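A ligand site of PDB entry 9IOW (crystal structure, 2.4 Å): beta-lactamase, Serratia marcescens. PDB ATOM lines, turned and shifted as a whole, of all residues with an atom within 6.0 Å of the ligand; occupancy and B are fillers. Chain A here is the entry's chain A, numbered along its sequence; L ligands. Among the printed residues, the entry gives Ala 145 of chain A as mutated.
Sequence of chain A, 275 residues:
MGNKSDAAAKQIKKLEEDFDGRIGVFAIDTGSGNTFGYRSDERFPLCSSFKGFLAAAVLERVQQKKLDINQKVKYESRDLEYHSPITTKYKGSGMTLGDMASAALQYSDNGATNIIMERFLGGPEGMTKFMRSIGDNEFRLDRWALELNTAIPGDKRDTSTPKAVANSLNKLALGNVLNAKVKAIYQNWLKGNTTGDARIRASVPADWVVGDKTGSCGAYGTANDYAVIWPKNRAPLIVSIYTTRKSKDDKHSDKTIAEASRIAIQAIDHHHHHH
Merely in contact with the ligand: Cys 47, Tyr 82, Gly 215 and Thr 195. Hydrophobic or aromatic side chains that line the ligand: Tyr 82 and His 83. Along chain A the residues within 4 Å of the ligand span positions 47 to 217.
N of Ser 48 sits at hydrogen-bond distance from O4 of the ligand, 2.6 Å away. The side-chain hydroxyl (OG) of Ser 48 is covalently linked to a carbon (C15) of the ligand (1.4 Å). The side-chain hydroxyl of Ser 108 sits at hydrogen-bond distance from a nitrogen (N3) of the ligand. OG1 of Thr 214 lies within hydrogen-bond range of O3 of the ligand. O4 of the ligand lies within hydrogen-bond range of N of Ser 216, 3.0 Å away. The backbone carbonyl oxygen (O) of Ser 216 lies within hydrogen-bond range of a nitrogen (N2) of the ligand (2.7 Å). OG of Ser 216 is in hydrogen-bond range of O2 of the ligand, 2.8 Å away. The side-chain amide nitrogen (ND2) of Asn 110 sits at hydrogen-bond distance from an oxygen (O1) of the ligand, at 3.0 Å. The side-chain amino group (NZ) of Lys 213 lies within salt-bridge range of an oxygen (O3) of the ligand. A ring nitrogen (NE2) of His 83 sits close to a sulfur (S1) of the ligand, 3.5 Å away. O1 of the ligand is in hydrogen-bond range of ND2 of Asn 149. The backbone carbonyl oxygen of Cys 217 is in hydrogen-bond range of a nitrogen (N1) of the ligand, at 3.5 Å.
O of Ser 108 lies close to NE2 of His 83, at 3.3 Å. The side-chain hydroxyl (OG1) of Thr 214 lies within hydrogen-bond range of the side-chain hydroxyl (OG1) of Thr 195, 2.7 Å away. O of Tyr 82 is in hydrogen-bond range of ND2 of Asn 110 (2.8 Å). OD1 of Asn 110 lies within hydrogen-bond range of NZ of Lys 51, at 3.1 Å. The side-chain sulfur (SG) of Cys 217 is disulfide-bonded to the side-chain sulfur (SG) of Cys 47 (2.2 Å). NE2 of His 83 is in hydrogen-bond range of O of Tyr 107 (3.0 Å). The side-chain amide oxygen (OD1) of Asn 149 sits close to the side-chain sulfur (SG) of Cys 217 (3.6 Å). The backbone carbonyl oxygen (O) of Gly 215 lies within hydrogen-bond range of the backbone NH (N) of Asn 224 (2.8 Å).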
ATOM      1  N   LEU A  46      19.580 -13.847  13.543  1.00  0.00           N
ATOM      2  CA  LEU A  46      19.274 -15.125  12.957  1.00  0.00           C
ATOM      3  C   LEU A  46      19.081 -16.191  14.042  1.00  0.00           C
ATOM      4  O   LEU A  46      18.244 -17.058  13.872  1.00  0.00           O
ATOM      5  CB  LEU A  46      20.309 -15.558  11.951  1.00  0.00           C
ATOM      6  CG  LEU A  46      20.388 -14.700  10.680  1.00  0.00           C
ATOM      7  CD1 LEU A  46      21.629 -15.082   9.800  1.00  0.00           C
ATOM      8  CD2 LEU A  46      19.100 -14.717   9.909  1.00  0.00           C
ATOM      9  N   CYS A  47      19.865 -16.144  15.143  1.00  0.00           N
ATOM     10  CA  CYS A  47      20.065 -17.333  15.977  1.00  0.00           C
ATOM     11  C   CYS A  47      20.335 -18.543  15.056  1.00  0.00           C
ATOM     12  O   CYS A  47      21.088 -18.422  14.102  1.00  0.00           O
ATOM     13  CB  CYS A  47      18.944 -17.527  16.996  1.00  0.00           C
ATOM     14  SG  CYS A  47      18.134 -15.975  17.499  1.00  0.00           S
ATOM     15  N   SER A  48      19.770 -19.710  15.388  1.00  0.00           N
ATOM     16  CA  SER A  48      20.047 -21.008  14.771  1.00  0.00           C
ATOM     17  C   SER A  48      19.468 -21.083  13.362  1.00  0.00           C
ATOM     18  O   SER A  48      19.694 -22.033  12.623  1.00  0.00           O
ATOM     19  CB  SER A  48      19.561 -22.159  15.599  1.00  0.00           C
ATOM     20  OG  SER A  48      20.395 -22.253  16.730  1.00  0.00           O
ATOM     21  N   SER A  49      18.670 -20.066  13.027  1.00  0.00           N
ATOM     22  CA  SER A  49      17.730 -20.282  11.964  1.00  0.00           C
ATOM     23  C   SER A  49      18.507 -20.290  10.639  1.00  0.00           C
ATOM     24  O   SER A  49      17.986 -20.742   9.617  1.00  0.00           O
ATOM     25  CB  SER A  49      16.503 -19.326  12.051  1.00  0.00           C
ATOM     26  OG  SER A  49      16.726 -18.046  11.505  1.00  0.00           O
ATOM     27  N   LYS A  51      20.649 -22.236   9.925  1.00  0.00           N
ATOM     28  CA  LYS A  51      21.031 -23.631   9.752  1.00  0.00           C
ATOM     29  C   LYS A  51      20.224 -24.347   8.675  1.00  0.00           C
ATOM     30  O   LYS A  51      20.770 -25.274   8.012  1.00  0.00           O
ATOM     31  CB  LYS A  51      20.914 -24.416  11.056  1.00  0.00           C
ATOM     32  CG  LYS A  51      22.109 -24.293  12.008  1.00  0.00           C
ATOM     33  CD  LYS A  51      21.606 -24.549  13.425  1.00  0.00           C
ATOM     34  CE  LYS A  51      22.503 -24.153  14.578  1.00  0.00           C
ATOM     35  NZ  LYS A  51      22.172 -24.912  15.795  1.00  0.00           N
ATOM     36  N   TYR A  82      28.279 -26.852  23.064  1.00  0.00           N
ATOM     37  CA  TYR A  82      27.062 -26.977  23.821  1.00  0.00           C
ATOM     38  C   TYR A  82      25.881 -27.032  22.864  1.00  0.00           C
ATOM     39  O   TYR A  82      25.833 -26.289  21.867  1.00  0.00           O
ATOM     40  CB  TYR A  82      26.942 -25.673  24.642  1.00  0.00           C
ATOM     41  CG  TYR A  82      25.638 -25.542  25.426  1.00  0.00           C
ATOM     42  CD1 TYR A  82      25.389 -26.348  26.544  1.00  0.00           C
ATOM     43  CD2 TYR A  82      24.679 -24.620  25.044  1.00  0.00           C
ATOM     44  CE1 TYR A  82      24.218 -26.208  27.277  1.00  0.00           C
ATOM     45  CE2 TYR A  82      23.489 -24.499  25.753  1.00  0.00           C
ATOM     46  CZ  TYR A  82      23.259 -25.300  26.844  1.00  0.00           C
ATOM     47  OH  TYR A  82      22.100 -25.185  27.552  1.00  0.00           O
ATOM     48  N   HIS A  83      24.913 -27.900  23.212  1.00  0.00           N
ATOM     49  CA  HIS A  83      23.694 -28.195  22.465  1.00  0.00           C
ATOM     50  C   HIS A  83      24.041 -28.824  21.109  1.00  0.00           C
ATOM     51  O   HIS A  83      23.653 -28.281  20.067  1.00  0.00           O
ATOM     52  CB  HIS A  83      22.773 -26.989  22.251  1.00  0.00           C
ATOM     53  CG  HIS A  83      21.455 -27.360  21.698  1.00  0.00           C
ATOM     54  ND1 HIS A  83      20.376 -27.675  22.483  1.00  0.00           N
ATOM     55  CD2 HIS A  83      21.089 -27.631  20.419  1.00  0.00           C
ATOM     56  CE1 HIS A  83      19.364 -28.026  21.712  1.00  0.00           C
ATOM     57  NE2 HIS A  83      19.776 -27.984  20.446  1.00  0.00           N
ATOM     58  N   LEU A 105      20.094 -29.022  10.944  1.00  0.00           N
ATOM     59  CA  LEU A 105      18.739 -28.540  10.681  1.00  0.00           C
ATOM     60  C   LEU A 105      17.764 -28.908  11.821  1.00  0.00           C
ATOM     61  O   LEU A 105      17.330 -28.037  12.572  1.00  0.00           O
ATOM     62  CB  LEU A 105      18.151 -28.835   9.309  1.00  0.00           C
ATOM     63  CG  LEU A 105      17.065 -27.866   8.807  1.00  0.00           C
ATOM     64  CD1 LEU A 105      16.928 -27.939   7.277  1.00  0.00           C
ATOM     65  CD2 LEU A 105      15.843 -28.402   9.422  1.00  0.00           C
ATOM     66  N   TYR A 107      17.597 -30.547  14.757  1.00  0.00           N
ATOM     67  CA  TYR A 107      17.802 -30.548  16.178  1.00  0.00           C
ATOM     68  C   TYR A 107      18.590 -29.312  16.587  1.00  0.00           C
ATOM     69  O   TYR A 107      18.864 -29.132  17.793  1.00  0.00           O
ATOM     70  CB  TYR A 107      18.686 -31.758  16.488  1.00  0.00           C
ATOM     71  CG  TYR A 107      17.860 -33.028  16.313  1.00  0.00           C
ATOM     72  CD1 TYR A 107      17.736 -33.602  15.063  1.00  0.00           C
ATOM     73  CD2 TYR A 107      17.166 -33.604  17.364  1.00  0.00           C
ATOM     74  CE1 TYR A 107      16.966 -34.714  14.828  1.00  0.00           C
ATOM     75  CE2 TYR A 107      16.377 -34.720  17.157  1.00  0.00           C
ATOM     76  CZ  TYR A 107      16.312 -35.287  15.889  1.00  0.00           C
ATOM     77  OH  TYR A 107      15.610 -36.408  15.589  1.00  0.00           O
ATOM     78  N   SER A 108      18.986 -28.518  15.579  1.00  0.00           N
ATOM     79  CA  SER A 108      19.779 -27.328  15.818  1.00  0.00           C
ATOM     80  C   SER A 108      21.073 -27.713  16.573  1.00  0.00           C
ATOM     81  O   SER A 108      21.367 -27.158  17.649  1.00  0.00           O
ATOM     82  CB  SER A 108      18.929 -26.269  16.566  1.00  0.00           C
ATOM     83  OG  SER A 108      19.191 -24.950  16.097  1.00  0.00           O
ATOM     84  N   ASN A 110      24.772 -27.632  17.418  1.00  0.00           N
ATOM     85  CA  ASN A 110      25.796 -26.612  17.197  1.00  0.00           C
ATOM     86  C   ASN A 110      27.133 -27.151  16.633  1.00  0.00           C
ATOM     87  O   ASN A 110      27.794 -26.487  15.801  1.00  0.00           O
ATOM     88  CB  ASN A 110      26.051 -25.680  18.399  1.00  0.00           C
ATOM     89  CG  ASN A 110      24.907 -24.723  18.684  1.00  0.00           C
ATOM     90  OD1 ASN A 110      24.341 -24.058  17.800  1.00  0.00           O
ATOM     91  ND2 ASN A 110      24.517 -24.669  19.931  1.00  0.00           N
ATOM     92  N   ALA A 145      28.719 -20.878  15.812  1.00  0.00           N
ATOM     93  CA  ALA A 145      27.380 -21.318  16.187  1.00  0.00           C
ATOM     94  C   ALA A 145      26.999 -20.782  17.568  1.00  0.00           C
ATOM     95  O   ALA A 145      25.819 -20.528  17.826  1.00  0.00           O
ATOM     96  CB  ALA A 145      27.361 -22.821  16.180  1.00  0.00           C
ATOM     97  N   LEU A 146      27.961 -20.597  18.454  1.00  0.00           N
ATOM     98  CA  LEU A 146      27.566 -20.064  19.770  1.00  0.00           C
ATOM     99  C   LEU A 146      27.628 -18.545  19.827  1.00  0.00           C
ATOM    100  O   LEU A 146      26.621 -17.909  20.168  1.00  0.00           O
ATOM    101  CB  LEU A 146      28.076 -20.778  21.021  1.00  0.00           C
ATOM    102  CG  LEU A 146      27.478 -22.191  21.150  1.00  0.00           C
ATOM    103  CD1 LEU A 146      28.598 -23.048  21.605  1.00  0.00           C
ATOM    104  CD2 LEU A 146      26.296 -22.368  22.100  1.00  0.00           C
ATOM    105  N   LEU A 148      27.108 -16.318  17.920  1.00  0.00           N
ATOM    106  CA  LEU A 148      26.245 -15.518  17.059  1.00  0.00           C
ATOM    107  C   LEU A 148      24.928 -15.248  17.758  1.00  0.00           C
ATOM    108  O   LEU A 148      24.062 -14.585  17.206  1.00  0.00           O
ATOM    109  CB  LEU A 148      26.036 -16.109  15.645  1.00  0.00           C
ATOM    110  CG  LEU A 148      25.462 -17.535  15.563  1.00  0.00           C
ATOM    111  CD1 LEU A 148      23.919 -17.631  15.759  1.00  0.00           C
ATOM    112  CD2 LEU A 148      25.999 -18.391  14.400  1.00  0.00           C
ATOM    113  N   ASN A 149      24.746 -15.816  18.944  1.00  0.00           N
ATOM    114  CA  ASN A 149      23.482 -15.820  19.684  1.00  0.00           C
ATOM    115  C   ASN A 149      23.446 -14.727  20.751  1.00  0.00           C
ATOM    116  O   ASN A 149      22.630 -14.809  21.653  1.00  0.00           O
ATOM    117  CB  ASN A 149      23.298 -17.166  20.393  1.00  0.00           C
ATOM    118  CG  ASN A 149      22.818 -18.244  19.457  1.00  0.00           C
ATOM    119  OD1 ASN A 149      21.725 -18.099  18.889  1.00  0.00           O
ATOM    120  ND2 ASN A 149      23.605 -19.293  19.264  1.00  0.00           N
ATOM    121  N   THR A 195      12.167 -29.003  16.392  1.00  0.00           N
ATOM    122  CA  THR A 195      12.256 -27.987  17.448  1.00  0.00           C
ATOM    123  C   THR A 195      11.131 -26.951  17.405  1.00  0.00           C
ATOM    124  O   THR A 195      11.151 -26.005  18.205  1.00  0.00           O
ATOM    125  CB  THR A 195      13.610 -27.273  17.434  1.00  0.00           C
ATOM    126  OG1 THR A 195      13.576 -26.693  16.121  1.00  0.00           O
ATOM    127  CG2 THR A 195      14.740 -28.205  17.880  1.00  0.00           C
ATOM    128  N   ARG A 199       5.667 -23.243  17.552  1.00  0.00           N
ATOM    129  CA  ARG A 199       5.773 -22.020  16.777  1.00  0.00           C
ATOM    130  C   ARG A 199       4.842 -22.056  15.567  1.00  0.00           C
ATOM    131  O   ARG A 199       3.650 -22.140  15.795  1.00  0.00           O
ATOM    132  CB  ARG A 199       7.270 -21.753  16.557  1.00  0.00           C
ATOM    133  CG  ARG A 199       7.880 -21.493  17.939  1.00  0.00           C
ATOM    134  CD  ARG A 199       9.334 -21.401  17.836  1.00  0.00           C
ATOM    135  NE  ARG A 199      10.010 -21.305  19.132  1.00  0.00           N
ATOM    136  CZ  ARG A 199      11.284 -20.844  19.205  1.00  0.00           C
ATOM    137  NH1 ARG A 199      11.957 -20.397  18.145  1.00  0.00           N
ATOM    138  NH2 ARG A 199      11.918 -20.742  20.354  1.00  0.00           N
ATOM    139  N   LYS A 213      12.554 -24.208  10.295  1.00  0.00           N
ATOM    140  CA  LYS A 213      13.783 -24.057  11.064  1.00  0.00           C
ATOM    141  C   LYS A 213      13.510 -22.953  12.041  1.00  0.00           C
ATOM    142  O   LYS A 213      13.191 -21.872  11.576  1.00  0.00           O
ATOM    143  CB  LYS A 213      15.077 -23.681  10.302  1.00  0.00           C
ATOM    144  CG  LYS A 213      16.378 -23.755  11.120  1.00  0.00           C
ATOM    145  CD  LYS A 213      16.830 -25.096  11.736  1.00  0.00           C
ATOM    146  CE  LYS A 213      17.846 -24.995  12.834  1.00  0.00           C
ATOM    147  NZ  LYS A 213      17.164 -24.824  14.149  1.00  0.00           N
ATOM    148  N   THR A 214      13.694 -23.259  13.333  1.00  0.00           N
ATOM    149  CA  THR A 214      13.563 -22.298  14.426  1.00  0.00           C
ATOM    150  C   THR A 214      14.942 -21.703  14.746  1.00  0.00           C
ATOM    151  O   THR A 214      15.981 -22.154  14.252  1.00  0.00           O
ATOM    152  CB  THR A 214      13.005 -23.042  15.637  1.00  0.00           C
ATOM    153  OG1 THR A 214      13.972 -24.066  15.921  1.00  0.00           O
ATOM    154  CG2 THR A 214      11.579 -23.490  15.359  1.00  0.00           C
ATOM    155  N   GLY A 215      14.945 -20.643  15.526  1.00  0.00           N
ATOM    156  CA  GLY A 215      16.162 -20.161  16.174  1.00  0.00           C
ATOM    157  C   GLY A 215      15.775 -19.604  17.551  1.00  0.00           C
ATOM    158  O   GLY A 215      14.658 -19.076  17.683  1.00  0.00           O
ATOM    159  N   SER A 216      16.697 -19.729  18.532  1.00  0.00           N
ATOM    160  CA  SER A 216      16.461 -19.345  19.938  1.00  0.00           C
ATOM    161  C   SER A 216      17.786 -18.927  20.570  1.00  0.00           C
ATOM    162  O   SER A 216      18.576 -19.791  20.996  1.00  0.00           O
ATOM    163  CB  SER A 216      15.863 -20.461  20.775  1.00  0.00           C
ATOM    164  OG  SER A 216      14.643 -20.970  20.275  1.00  0.00           O
ATOM    165  N   CYS A 217      18.000 -17.589  20.564  1.00  0.00           N
ATOM    166  CA  CYS A 217      19.260 -16.956  20.921  1.00  0.00           C
ATOM    167  C   CYS A 217      19.507 -17.156  22.401  1.00  0.00           C
ATOM    168  O   CYS A 217      20.645 -17.333  22.819  1.00  0.00           O
ATOM    169  CB  CYS A 217      19.266 -15.460  20.584  1.00  0.00           C
ATOM    170  SG  CYS A 217      19.656 -15.107  18.834  1.00  0.00           S
ATOM    171  N   GLY A 218      18.404 -17.233  23.159  1.00  0.00           N
ATOM    172  CA  GLY A 218      18.467 -17.285  24.605  1.00  0.00           C
ATOM    173  C   GLY A 218      18.980 -15.993  25.250  1.00  0.00           C
ATOM    174  O   GLY A 218      19.514 -16.070  26.337  1.00  0.00           O
ATOM    175  N   ASN A 224      12.843 -17.130  16.680  1.00  0.00           N
ATOM    176  CA  ASN A 224      12.228 -16.962  15.374  1.00  0.00           C
ATOM    177  C   ASN A 224      11.786 -18.331  14.840  1.00  0.00           C
ATOM    178  O   ASN A 224      11.959 -19.388  15.474  1.00  0.00           O
ATOM    179  CB  ASN A 224      13.201 -16.195  14.470  1.00  0.00           C
ATOM    180  CG  ASN A 224      14.570 -16.854  14.605  1.00  0.00           C
ATOM    181  OD1 ASN A 224      14.718 -18.023  14.240  1.00  0.00           O
ATOM    182  ND2 ASN A 224      15.517 -16.220  15.301  1.00  0.00           N
ATOM    183  N   HIS A 252      12.039 -15.867  25.607  1.00  0.00           N
ATOM    184  CA  HIS A 252      11.470 -15.824  24.277  1.00  0.00           C
ATOM    185  C   HIS A 252      10.044 -16.302  24.481  1.00  0.00           C
ATOM    186  O   HIS A 252       9.768 -16.881  25.541  1.00  0.00           O
ATOM    187  CB  HIS A 252      12.282 -16.690  23.296  1.00  0.00           C
ATOM    188  CG  HIS A 252      12.286 -18.163  23.571  1.00  0.00           C
ATOM    189  ND1 HIS A 252      13.461 -18.883  23.605  1.00  0.00           N
ATOM    190  CD2 HIS A 252      11.301 -19.078  23.797  1.00  0.00           C
ATOM    191  CE1 HIS A 252      13.199 -20.181  23.853  1.00  0.00           C
ATOM    192  NE2 HIS A 252      11.908 -20.335  23.973  1.00  0.00           N
HETATM  193  C1  LIG L   1      18.786 -21.342  24.541  1.00  0.00           C
HETATM  194  C2  LIG L   1      20.108 -22.241  19.162  1.00  0.00           C
HETATM  195  C3  LIG L   1      16.282 -23.662  18.157  1.00  0.00           C
HETATM  196  C4  LIG L   1      19.840 -21.026  23.697  1.00  0.00           C
HETATM  197  C5  LIG L   1      19.972 -23.743  19.001  1.00  0.00           C
HETATM  198  C6  LIG L   1      20.783 -21.993  23.407  1.00  0.00           C
HETATM  199  C7  LIG L   1      20.684 -23.299  23.945  1.00  0.00           C
HETATM  200  C8  LIG L   1      18.424 -23.669  21.395  1.00  0.00           C
HETATM  201  C9  LIG L   1      19.630 -23.615  24.789  1.00  0.00           C
HETATM  202  C10 LIG L   1      17.291 -23.686  20.516  1.00  0.00           C
HETATM  203  C11 LIG L   1      18.690 -22.617  25.087  1.00  0.00           C
HETATM  204  C12 LIG L   1      17.494 -23.701  19.052  1.00  0.00           C
HETATM  205  C13 LIG L   1      21.921 -21.682  22.480  1.00  0.00           C
HETATM  206  C14 LIG L   1      21.684 -21.905  20.988  1.00  0.00           C
HETATM  207  C15 LIG L   1      20.335 -21.488  17.857  1.00  0.00           C
HETATM  208  N1  LIG L   1      22.432 -20.311  22.605  1.00  0.00           N
HETATM  209  N2  LIG L   1      20.516 -21.631  20.435  1.00  0.00           N
HETATM  210  N3  LIG L   1      18.662 -23.784  18.373  1.00  0.00           N
HETATM  211  O1  LIG L   1      22.598 -22.354  20.339  1.00  0.00           O
HETATM  212  O2  LIG L   1      15.285 -23.097  18.645  1.00  0.00           O
HETATM  213  O3  LIG L   1      16.403 -24.244  17.041  1.00  0.00           O
HETATM  214  S1  LIG L   1      19.844 -24.494  20.682  1.00  0.00           S
HETATM  215 CL1  LIG L   1      15.832 -23.610  21.488  1.00  0.00          CL
HETATM  216  O4  LIG L   1      19.548 -20.576  17.882  1.00  0.00           O
